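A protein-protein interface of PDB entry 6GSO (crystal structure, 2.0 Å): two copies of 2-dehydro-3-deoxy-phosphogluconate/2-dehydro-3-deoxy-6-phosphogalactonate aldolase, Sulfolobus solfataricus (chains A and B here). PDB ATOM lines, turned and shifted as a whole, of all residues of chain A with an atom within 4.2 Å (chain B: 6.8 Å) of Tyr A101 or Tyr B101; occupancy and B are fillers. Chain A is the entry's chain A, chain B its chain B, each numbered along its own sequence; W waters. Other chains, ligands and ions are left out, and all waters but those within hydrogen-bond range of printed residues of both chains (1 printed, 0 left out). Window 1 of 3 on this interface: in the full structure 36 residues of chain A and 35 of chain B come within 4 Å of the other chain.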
ATOM      1  N   PRO A  47      -2.900   4.244   2.367  1.00  0.00           N
ATOM      2  CA  PRO A  47      -2.243   4.822   1.187  1.00  0.00           C
ATOM      3  C   PRO A  47      -3.219   5.367   0.180  1.00  0.00           C
ATOM      4  O   PRO A  47      -2.848   6.236  -0.609  1.00  0.00           O
ATOM      5  CB  PRO A  47      -1.438   3.640   0.626  1.00  0.00           C
ATOM      6  CG  PRO A  47      -1.130   2.847   1.819  1.00  0.00           C
ATOM      7  CD  PRO A  47      -2.348   2.915   2.682  1.00  0.00           C
ATOM      8  N   LEU A  75       4.092   9.920   1.021  1.00  0.00           N
ATOM      9  CA  LEU A  75       5.208  10.342   0.190  1.00  0.00           C
ATOM     10  C   LEU A  75       5.380  11.849   0.139  1.00  0.00           C
ATOM     11  O   LEU A  75       6.234  12.343  -0.607  1.00  0.00           O
ATOM     12  CB  LEU A  75       5.040   9.784  -1.231  1.00  0.00           C
ATOM     13  CG  LEU A  75       5.059   8.253  -1.322  1.00  0.00           C
ATOM     14  CD1 LEU A  75       4.829   7.815  -2.770  1.00  0.00           C
ATOM     15  CD2 LEU A  75       6.376   7.679  -0.800  1.00  0.00           C
ATOM     16  N   TYR A  98       4.409   4.064   8.241  1.00  0.00           N
ATOM     17  CA  TYR A  98       5.192   3.123   7.448  1.00  0.00           C
ATOM     18  C   TYR A  98       6.349   3.858   6.807  1.00  0.00           C
ATOM     19  O   TYR A  98       6.372   5.090   6.741  1.00  0.00           O
ATOM     20  CB  TYR A  98       4.393   2.425   6.332  1.00  0.00           C
ATOM     21  CG  TYR A  98       3.207   3.155   5.773  1.00  0.00           C
ATOM     22  CD1 TYR A  98       3.344   4.400   5.189  1.00  0.00           C
ATOM     23  CD2 TYR A  98       1.949   2.578   5.793  1.00  0.00           C
ATOM     24  CE1 TYR A  98       2.275   5.058   4.685  1.00  0.00           C
ATOM     25  CE2 TYR A  98       0.871   3.231   5.287  1.00  0.00           C
ATOM     26  CZ  TYR A  98       1.034   4.481   4.744  1.00  0.00           C
ATOM     27  OH  TYR A  98      -0.046   5.167   4.229  1.00  0.00           O
ATOM     28  N   ALA A  99       7.322   3.078   6.342  1.00  0.00           N
ATOM     29  CA  ALA A  99       8.404   3.626   5.564  1.00  0.00           C
ATOM     30  C   ALA A  99       7.822   4.210   4.294  1.00  0.00           C
ATOM     31  O   ALA A  99       6.789   3.731   3.806  1.00  0.00           O
ATOM     32  CB  ALA A  99       9.430   2.543   5.205  1.00  0.00           C
ATOM     33  N   PRO A 100       8.439   5.261   3.756  1.00  0.00           N
ATOM     34  CA  PRO A 100       8.095   5.710   2.406  1.00  0.00           C
ATOM     35  C   PRO A 100       8.064   4.525   1.459  1.00  0.00           C
ATOM     36  O   PRO A 100       9.003   3.708   1.411  1.00  0.00           O
ATOM     37  CB  PRO A 100       9.221   6.685   2.054  1.00  0.00           C
ATOM     38  CG  PRO A 100       9.772   7.112   3.349  1.00  0.00           C
ATOM     39  CD  PRO A 100       9.604   5.977   4.302  1.00  0.00           C
ATOM     40  N   TYR A 101       6.961   4.404   0.738  1.00  0.00           N
ATOM     41  CA  TYR A 101       6.706   3.212  -0.045  1.00  0.00           C
ATOM     42  C   TYR A 101       7.007   3.495  -1.512  1.00  0.00           C
ATOM     43  O   TYR A 101       7.403   4.601  -1.895  1.00  0.00           O
ATOM     44  CB  TYR A 101       5.265   2.733   0.147  1.00  0.00           C
ATOM     45  CG  TYR A 101       4.195   3.798   0.021  1.00  0.00           C
ATOM     46  CD1 TYR A 101       3.717   4.220  -1.225  1.00  0.00           C
ATOM     47  CD2 TYR A 101       3.633   4.359   1.159  1.00  0.00           C
ATOM     48  CE1 TYR A 101       2.712   5.200  -1.307  1.00  0.00           C
ATOM     49  CE2 TYR A 101       2.656   5.311   1.077  1.00  0.00           C
ATOM     50  CZ  TYR A 101       2.186   5.727  -0.139  1.00  0.00           C
ATOM     51  OH  TYR A 101       1.192   6.714  -0.130  1.00  0.00           O
ATOM     52  N   TYR A 102       6.815   2.469  -2.335  1.00  0.00           N
ATOM     53  CA  TYR A 102       7.014   2.565  -3.773  1.00  0.00           C
ATOM     54  C   TYR A 102       8.500   2.655  -4.120  1.00  0.00           C
ATOM     55  O   TYR A 102       9.017   1.786  -4.834  1.00  0.00           O
ATOM     56  CB  TYR A 102       6.242   3.757  -4.365  1.00  0.00           C
ATOM     57  CG  TYR A 102       6.308   3.799  -5.866  1.00  0.00           C
ATOM     58  CD1 TYR A 102       7.429   4.318  -6.513  1.00  0.00           C
ATOM     59  CD2 TYR A 102       5.271   3.307  -6.639  1.00  0.00           C
ATOM     60  CE1 TYR A 102       7.520   4.337  -7.885  1.00  0.00           C
ATOM     61  CE2 TYR A 102       5.348   3.321  -8.033  1.00  0.00           C
ATOM     62  CZ  TYR A 102       6.480   3.843  -8.650  1.00  0.00           C
ATOM     63  OH  TYR A 102       6.595   3.880 -10.032  1.00  0.00           O
ATOM     64  N   TYR A 103       9.212   3.659  -3.616  1.00  0.00           N
ATOM     65  CA  TYR A 103      10.526   3.948  -4.191  1.00  0.00           C
ATOM     66  C   TYR A 103      11.541   2.890  -3.783  1.00  0.00           C
ATOM     67  O   TYR A 103      11.863   2.773  -2.592  1.00  0.00           O
ATOM     68  CB  TYR A 103      11.023   5.334  -3.791  1.00  0.00           C
ATOM     69  CG  TYR A 103      10.142   6.400  -4.359  1.00  0.00           C
ATOM     70  CD1 TYR A 103       9.987   6.550  -5.745  1.00  0.00           C
ATOM     71  CD2 TYR A 103       9.437   7.232  -3.525  1.00  0.00           C
ATOM     72  CE1 TYR A 103       9.139   7.539  -6.277  1.00  0.00           C
ATOM     73  CE2 TYR A 103       8.599   8.241  -4.034  1.00  0.00           C
ATOM     74  CZ  TYR A 103       8.438   8.375  -5.392  1.00  0.00           C
ATOM     75  OH  TYR A 103       7.591   9.345  -5.883  1.00  0.00           O
ATOM     76  N   THR A 135       5.782  -1.665   1.394  1.00  0.00           N
ATOM     77  CA  THR A 135       6.599  -0.470   1.153  1.00  0.00           C
ATOM     78  C   THR A 135       7.802  -0.742   0.259  1.00  0.00           C
ATOM     79  O   THR A 135       8.287   0.180  -0.404  1.00  0.00           O
ATOM     80  CB  THR A 135       7.137   0.126   2.463  1.00  0.00           C
ATOM     81  OG1 THR A 135       7.924  -0.845   3.177  1.00  0.00           O
ATOM     82  CG2 THR A 135       6.012   0.639   3.358  1.00  0.00           C
ATOM     83  N   LYS A 137      10.706  -1.959   1.686  1.00  0.00           N
ATOM     84  CA  LYS A 137      11.917  -1.968   2.499  1.00  0.00           C
ATOM     85  C   LYS A 137      11.549  -2.267   3.943  1.00  0.00           C
ATOM     86  O   LYS A 137      10.428  -2.008   4.385  1.00  0.00           O
ATOM     87  CB  LYS A 137      12.702  -0.652   2.406  1.00  0.00           C
ATOM     88  CG  LYS A 137      11.964   0.577   2.900  1.00  0.00           C
ATOM     89  CD  LYS A 137      10.954   1.121   1.875  1.00  0.00           C
ATOM     90  CE  LYS A 137      11.631   1.749   0.672  1.00  0.00           C
ATOM     91  NZ  LYS A 137      10.637   2.303  -0.277  1.00  0.00           N
ATOM     92  N   GLY B  46       6.291  10.689  -9.661  1.00  0.00           N
ATOM     93  CA  GLY B  46       4.895  10.503  -9.950  1.00  0.00           C
ATOM     94  C   GLY B  46       4.046  10.159  -8.731  1.00  0.00           C
ATOM     95  O   GLY B  46       3.014  10.795  -8.482  1.00  0.00           O
ATOM     96  N   PRO B  47       4.415   9.118  -7.977  1.00  0.00           N
ATOM     97  CA  PRO B  47       3.557   8.728  -6.837  1.00  0.00           C
ATOM     98  C   PRO B  47       3.529   9.761  -5.729  1.00  0.00           C
ATOM     99  O   PRO B  47       2.592   9.741  -4.927  1.00  0.00           O
ATOM    100  CB  PRO B  47       4.179   7.411  -6.339  1.00  0.00           C
ATOM    101  CG  PRO B  47       4.938   6.854  -7.539  1.00  0.00           C
ATOM    102  CD  PRO B  47       5.426   8.083  -8.287  1.00  0.00           C
ATOM    103  N   SER B  48       4.518  10.657  -5.658  1.00  0.00           N
ATOM    104  CA  SER B  48       4.511  11.724  -4.663  1.00  0.00           C
ATOM    105  C   SER B  48       3.691  12.919  -5.105  1.00  0.00           C
ATOM    106  O   SER B  48       3.595  13.898  -4.362  1.00  0.00           O
ATOM    107  CB  SER B  48       5.945  12.164  -4.363  1.00  0.00           C
ATOM    108  OG  SER B  48       6.783  11.027  -4.176  1.00  0.00           O
ATOM    109  N   LEU B  49       3.098  12.864  -6.291  1.00  0.00           N
ATOM    110  CA  LEU B  49       2.371  13.980  -6.855  1.00  0.00           C
ATOM    111  C   LEU B  49       0.878  13.767  -6.696  1.00  0.00           C
ATOM    112  O   LEU B  49       0.384  12.669  -6.937  1.00  0.00           O
ATOM    113  CB  LEU B  49       2.679  14.154  -8.341  1.00  0.00           C
ATOM    114  CG  LEU B  49       4.134  14.385  -8.757  1.00  0.00           C
ATOM    115  CD1 LEU B  49       4.269  14.674 -10.271  1.00  0.00           C
ATOM    116  CD2 LEU B  49       4.718  15.518  -7.959  1.00  0.00           C
ATOM    117  N   LYS B  54       0.133  16.292 -11.065  1.00  0.00           N
ATOM    118  CA  LYS B  54       0.410  15.470 -12.246  1.00  0.00           C
ATOM    119  C   LYS B  54       0.008  16.208 -13.512  1.00  0.00           C
ATOM    120  O   LYS B  54       0.708  16.149 -14.535  1.00  0.00           O
ATOM    121  CB  LYS B  54      -0.335  14.142 -12.153  1.00  0.00           C
ATOM    122  CG  LYS B  54       0.317  13.095 -11.246  1.00  0.00           C
ATOM    123  CD  LYS B  54      -0.365  11.733 -11.405  1.00  0.00           C
ATOM    124  CE  LYS B  54       0.325  10.638 -10.561  1.00  0.00           C
ATOM    125  NZ  LYS B  54       0.170  10.756  -9.030  1.00  0.00           N
ATOM    126  N   GLY B  73      -1.582   7.004 -13.128  1.00  0.00           N
ATOM    127  CA  GLY B  73      -2.105   6.051 -12.172  1.00  0.00           C
ATOM    128  C   GLY B  73      -1.993   6.496 -10.728  1.00  0.00           C
ATOM    129  O   GLY B  73      -1.249   7.405 -10.360  1.00  0.00           O
ATOM    130  N   GLY B  74      -2.737   5.783  -9.892  1.00  0.00           N
ATOM    131  CA  GLY B  74      -2.637   5.950  -8.456  1.00  0.00           C
ATOM    132  C   GLY B  74      -3.601   5.017  -7.761  1.00  0.00           C
ATOM    133  O   GLY B  74      -4.155   4.093  -8.370  1.00  0.00           O
ATOM    134  N   LEU B  75      -3.778   5.251  -6.464  1.00  0.00           N
ATOM    135  CA  LEU B  75      -4.590   4.383  -5.629  1.00  0.00           C
ATOM    136  C   LEU B  75      -6.007   4.907  -5.455  1.00  0.00           C
ATOM    137  O   LEU B  75      -6.738   4.452  -4.562  1.00  0.00           O
ATOM    138  CB  LEU B  75      -3.922   4.182  -4.267  1.00  0.00           C
ATOM    139  CG  LEU B  75      -2.577   3.447  -4.302  1.00  0.00           C
ATOM    140  CD1 LEU B  75      -1.989   3.277  -2.883  1.00  0.00           C
ATOM    141  CD2 LEU B  75      -2.744   2.085  -4.987  1.00  0.00           C
ATOM    142  N   ASN B  76      -6.420   5.842  -6.299  1.00  0.00           N
ATOM    143  CA  ASN B  76      -7.817   6.247  -6.363  1.00  0.00           C
ATOM    144  C   ASN B  76      -8.173   6.270  -7.834  1.00  0.00           C
ATOM    145  O   ASN B  76      -7.740   7.158  -8.573  1.00  0.00           O
ATOM    146  CB  ASN B  76      -8.055   7.603  -5.692  1.00  0.00           C
ATOM    147  CG  ASN B  76      -9.487   8.074  -5.834  1.00  0.00           C
ATOM    148  OD1 ASN B  76     -10.024   8.123  -6.927  1.00  0.00           O
ATOM    149  ND2 ASN B  76     -10.109   8.400  -4.731  1.00  0.00           N
ATOM    150  N   TYR B  98       1.338   2.680 -14.021  1.00  0.00           N
ATOM    151  CA  TYR B  98       1.782   1.510 -13.270  1.00  0.00           C
ATOM    152  C   TYR B  98       0.616   0.811 -12.605  1.00  0.00           C
ATOM    153  O   TYR B  98      -0.486   1.346 -12.449  1.00  0.00           O
ATOM    154  CB  TYR B  98       2.803   1.860 -12.190  1.00  0.00           C
ATOM    155  CG  TYR B  98       2.636   3.237 -11.565  1.00  0.00           C
ATOM    156  CD1 TYR B  98       1.467   3.586 -10.957  1.00  0.00           C
ATOM    157  CD2 TYR B  98       3.677   4.170 -11.590  1.00  0.00           C
ATOM    158  CE1 TYR B  98       1.315   4.839 -10.379  1.00  0.00           C
ATOM    159  CE2 TYR B  98       3.551   5.384 -11.044  1.00  0.00           C
ATOM    160  CZ  TYR B  98       2.362   5.731 -10.425  1.00  0.00           C
ATOM    161  OH  TYR B  98       2.225   6.987  -9.877  1.00  0.00           O
ATOM    162  N   ALA B  99       0.885  -0.404 -12.179  1.00  0.00           N
ATOM    163  CA  ALA B  99      -0.113  -1.125 -11.434  1.00  0.00           C
ATOM    164  C   ALA B  99      -0.296  -0.451 -10.078  1.00  0.00           C
ATOM    165  O   ALA B  99       0.603   0.252  -9.597  1.00  0.00           O
ATOM    166  CB  ALA B  99       0.286  -2.584 -11.243  1.00  0.00           C
ATOM    167  N   PRO B 100      -1.456  -0.615  -9.475  1.00  0.00           N
ATOM    168  CA  PRO B 100      -1.655  -0.172  -8.093  1.00  0.00           C
ATOM    169  C   PRO B 100      -0.563  -0.658  -7.162  1.00  0.00           C
ATOM    170  O   PRO B 100      -0.375  -1.869  -6.951  1.00  0.00           O
ATOM    171  CB  PRO B 100      -3.016  -0.783  -7.728  1.00  0.00           C
ATOM    172  CG  PRO B 100      -3.731  -0.851  -9.042  1.00  0.00           C
ATOM    173  CD  PRO B 100      -2.669  -1.237 -10.028  1.00  0.00           C
ATOM    174  N   TYR B 101       0.130   0.305  -6.558  1.00  0.00           N
ATOM    175  CA  TYR B 101       1.283   0.008  -5.734  1.00  0.00           C
ATOM    176  C   TYR B 101       0.861  -0.249  -4.282  1.00  0.00           C
ATOM    177  O   TYR B 101      -0.311  -0.164  -3.908  1.00  0.00           O
ATOM    178  CB  TYR B 101       2.310   1.138  -5.846  1.00  0.00           C
ATOM    179  CG  TYR B 101       1.756   2.565  -5.823  1.00  0.00           C
ATOM    180  CD1 TYR B 101       1.543   3.243  -4.626  1.00  0.00           C
ATOM    181  CD2 TYR B 101       1.474   3.231  -7.013  1.00  0.00           C
ATOM    182  CE1 TYR B 101       1.039   4.568  -4.626  1.00  0.00           C
ATOM    183  CE2 TYR B 101       0.995   4.527  -7.024  1.00  0.00           C
ATOM    184  CZ  TYR B 101       0.781   5.185  -5.835  1.00  0.00           C
ATOM    185  OH  TYR B 101       0.300   6.452  -5.892  1.00  0.00           O
ATOM    186  N   TYR B 102       1.845  -0.595  -3.462  1.00  0.00           N
ATOM    187  CA  TYR B 102       1.683  -0.801  -2.025  1.00  0.00           C
ATOM    188  C   TYR B 102       0.942  -2.095  -1.698  1.00  0.00           C
ATOM    189  O   TYR B 102       1.498  -2.974  -1.033  1.00  0.00           O
ATOM    190  CB  TYR B 102       0.965   0.385  -1.369  1.00  0.00           C
ATOM    191  CG  TYR B 102       0.939   0.255   0.140  1.00  0.00           C
ATOM    192  CD1 TYR B 102      -0.038  -0.512   0.766  1.00  0.00           C
ATOM    193  CD2 TYR B 102       1.923   0.837   0.935  1.00  0.00           C
ATOM    194  CE1 TYR B 102      -0.064  -0.678   2.149  1.00  0.00           C
ATOM    195  CE2 TYR B 102       1.908   0.685   2.346  1.00  0.00           C
ATOM    196  CZ  TYR B 102       0.902  -0.076   2.942  1.00  0.00           C
ATOM    197  OH  TYR B 102       0.816  -0.254   4.320  1.00  0.00           O
ATOM    198  N   TYR B 103      -0.305  -2.224  -2.136  1.00  0.00           N
ATOM    199  CA  TYR B 103      -1.137  -3.335  -1.679  1.00  0.00           C
ATOM    200  C   TYR B 103      -0.618  -4.649  -2.255  1.00  0.00           C
ATOM    201  O   TYR B 103      -0.611  -4.822  -3.477  1.00  0.00           O
ATOM    202  CB  TYR B 103      -2.603  -3.117  -2.064  1.00  0.00           C
ATOM    203  CG  TYR B 103      -3.159  -1.876  -1.421  1.00  0.00           C
ATOM    204  CD1 TYR B 103      -3.170  -1.735  -0.031  1.00  0.00           C
ATOM    205  CD2 TYR B 103      -3.645  -0.845  -2.196  1.00  0.00           C
ATOM    206  CE1 TYR B 103      -3.666  -0.575   0.568  1.00  0.00           C
ATOM    207  CE2 TYR B 103      -4.126   0.288  -1.633  1.00  0.00           C
ATOM    208  CZ  TYR B 103      -4.136   0.436  -0.251  1.00  0.00           C
ATOM    209  OH  TYR B 103      -4.625   1.619   0.292  1.00  0.00           O
ATOM    210  N   PRO B 104      -0.190  -5.591  -1.429  1.00  0.00           N
ATOM    211  CA  PRO B 104       0.276  -6.879  -1.941  1.00  0.00           C
ATOM    212  C   PRO B 104      -0.892  -7.837  -2.131  1.00  0.00           C
ATOM    213  O   PRO B 104      -1.967  -7.669  -1.549  1.00  0.00           O
ATOM    214  CB  PRO B 104       1.218  -7.356  -0.833  1.00  0.00           C
ATOM    215  CG  PRO B 104       0.573  -6.818   0.431  1.00  0.00           C
ATOM    216  CD  PRO B 104      -0.213  -5.565   0.042  1.00  0.00           C
ATOM    217  N   MET B 106      -2.984  -8.406  -4.667  1.00  0.00           N
ATOM    218  CA  MET B 106      -4.206  -8.034  -5.362  1.00  0.00           C
ATOM    219  C   MET B 106      -4.475  -9.074  -6.442  1.00  0.00           C
ATOM    220  O   MET B 106      -3.545  -9.541  -7.105  1.00  0.00           O
ATOM    221  CB  MET B 106      -4.071  -6.662  -5.993  1.00  0.00           C
ATOM    222  CG  MET B 106      -3.666  -5.579  -5.040  1.00  0.00           C
ATOM    223  SD  MET B 106      -3.487  -4.015  -5.931  1.00  0.00           S
ATOM    224  CE  MET B 106      -5.090  -3.875  -6.755  1.00  0.00           C
ATOM    225  N   ALA B 134       8.741  -1.474  -7.638  1.00  0.00           N
ATOM    226  CA  ALA B 134       8.095  -0.352  -6.953  1.00  0.00           C
ATOM    227  C   ALA B 134       6.654  -0.675  -6.550  1.00  0.00           C
ATOM    228  O   ALA B 134       6.211  -0.304  -5.452  1.00  0.00           O
ATOM    229  CB  ALA B 134       8.123   0.902  -7.841  1.00  0.00           C
ATOM    230  N   THR B 135       5.910  -1.359  -7.420  1.00  0.00           N
ATOM    231  CA  THR B 135       4.501  -1.647  -7.177  1.00  0.00           C
ATOM    232  C   THR B 135       4.298  -2.929  -6.385  1.00  0.00           C
ATOM    233  O   THR B 135       3.253  -3.088  -5.742  1.00  0.00           O
ATOM    234  CB  THR B 135       3.721  -1.755  -8.506  1.00  0.00           C
ATOM    235  OG1 THR B 135       4.314  -2.753  -9.365  1.00  0.00           O
ATOM    236  CG2 THR B 135       3.653  -0.395  -9.224  1.00  0.00           C
ATOM    237  N   GLY B 136       5.276  -3.831  -6.411  1.00  0.00           N
ATOM    238  CA  GLY B 136       5.143  -5.115  -5.765  1.00  0.00           C
ATOM    239  C   GLY B 136       4.406  -6.149  -6.571  1.00  0.00           C
ATOM    240  O   GLY B 136       4.011  -7.177  -6.014  1.00  0.00           O
ATOM    241  N   LYS B 137       4.199  -5.913  -7.867  1.00  0.00           N
ATOM    242  CA  LYS B 137       3.534  -6.898  -8.710  1.00  0.00           C
ATOM    243  C   LYS B 137       3.924  -6.681 -10.159  1.00  0.00           C
ATOM    244  O   LYS B 137       4.168  -5.551 -10.596  1.00  0.00           O
ATOM    245  CB  LYS B 137       2.007  -6.854  -8.599  1.00  0.00           C
ATOM    246  CG  LYS B 137       1.361  -5.531  -9.009  1.00  0.00           C
ATOM    247  CD  LYS B 137       1.342  -4.518  -7.875  1.00  0.00           C
ATOM    248  CE  LYS B 137       0.554  -4.978  -6.630  1.00  0.00           C
ATOM    249  NZ  LYS B 137       0.541  -3.874  -5.623  1.00  0.00           N
ATOM    250  N   PRO B 262      10.051  12.617   1.335  1.00  0.00           N
ATOM    251  CA  PRO B 262      11.306  12.047   1.823  1.00  0.00           C
ATOM    252  C   PRO B 262      12.363  11.649   0.769  1.00  0.00           C
ATOM    253  O   PRO B 262      13.286  10.916   1.122  1.00  0.00           O
ATOM    254  CB  PRO B 262      10.834  10.790   2.560  1.00  0.00           C
ATOM    255  CG  PRO B 262       9.596  10.397   1.866  1.00  0.00           C
ATOM    256  CD  PRO B 262       8.921  11.696   1.563  1.00  0.00           C
HETATM  257  O   HOH W   1       8.498  12.089  -2.090  1.00  0.00           O
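OG of Ser B48 is in hydrogen-bond range of OH of Tyr A103.
The backbone carbonyl oxygen (O) of Tyr A103 lies within hydrogen-bond range of the side-chain amino group (NZ) of Lys A137 (2.7 Å). The backbone carbonyl oxygen (O) of Thr A135 sits at hydrogen-bond distance from the backbone NH (N) of Tyr A102 (3.3 Å). The side-chain amino group of Lys B137 sits at hydrogen-bond distance from the backbone carbonyl oxygen of Tyr B103, 2.6 Å away. NZ of Lys A137 sits at hydrogen-bond distance from O of Pro A100 (2.7 Å).
Among the printed residues, merely in contact across the chains: Tyr A102 with Ala B134, Tyr A102 with Tyr B98, Tyr A98 with Tyr B102, Tyr A103 with Pro B47, Leu A75 with Pro B262, Pro A47 with Tyr B103, Tyr A102 with Pro B47, Pro A47 with Leu B75, Pro A100 with Pro B262, Leu A75 with Ser B48, Leu A75 with Pro B47, Tyr A102 with Tyr B101, Pro A47 with Tyr B102, Tyr A101 with Tyr B101 and Tyr A101 with Tyr B102.
Printed residues of chain B within 4 Å of Leu A75: Pro B47 (3.7 Å), Ser B48 (3.6 Å) and Pro B262 (3.5 Å). Tyr A101 touches just these residues of chain B: Tyr B101 and Tyr B102. Thr A135 touches none of the printed residues of chain B. Printed residues of chain A within 4 Å of Ser B48: Leu A75 and Tyr A103. Ala B99 touches none of the printed residues of chain A. Printed residues of chain A within 4 Å of Tyr B101: Tyr A101 (3.8 Å) and Tyr A102 (3.7 Å). Printed residues of chain A within 4 Å of Tyr B103: Pro A47 (3.5 Å). The nearest printed residue of chain A that does not touch Tyr B101 is Leu A75 (5.3 Å).
Printed residues of chain B that touch a printed residue of chain A: Pro B47, Ser B48, Leu B75, Tyr B98, Tyr B101, Tyr B102, Tyr B103, Ala B134 and Pro B262. Hydrophobic or aromatic side chains of chain B within 4 Å of the printed part of chain A: Pro B47, Leu B75, Tyr B98, Tyr B101, Tyr B102, Tyr B103, Ala B134 and Pro B262. Of the 10 printed residues of chain A, 7 touch a printed residue of chain B. Among the printed residues, no Asp or Glu carboxylate lies within 4 Å of a Lys or Arg side-chain nitrogen of the other chain.
Pro A47 touches Leu B75, and with the chains exchanged Leu A75 touches Pro B47. Pro A47 touches Tyr B102, and with the chains exchanged Tyr A102 touches Pro B47. Tyr B101 touches its own counterpart, Tyr A101. Tyr A101 touches Tyr B102, and with the chains exchanged Tyr A102 touches Tyr B101. Positions printed for both chains: 47, 75, 98, 99, 100, 101, 102, 103, 135 and 137.
Water W1 lies within hydrogen-bond range of O of Leu A75 (2.7 Å) and OG of Ser B48 (2.9 Å).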
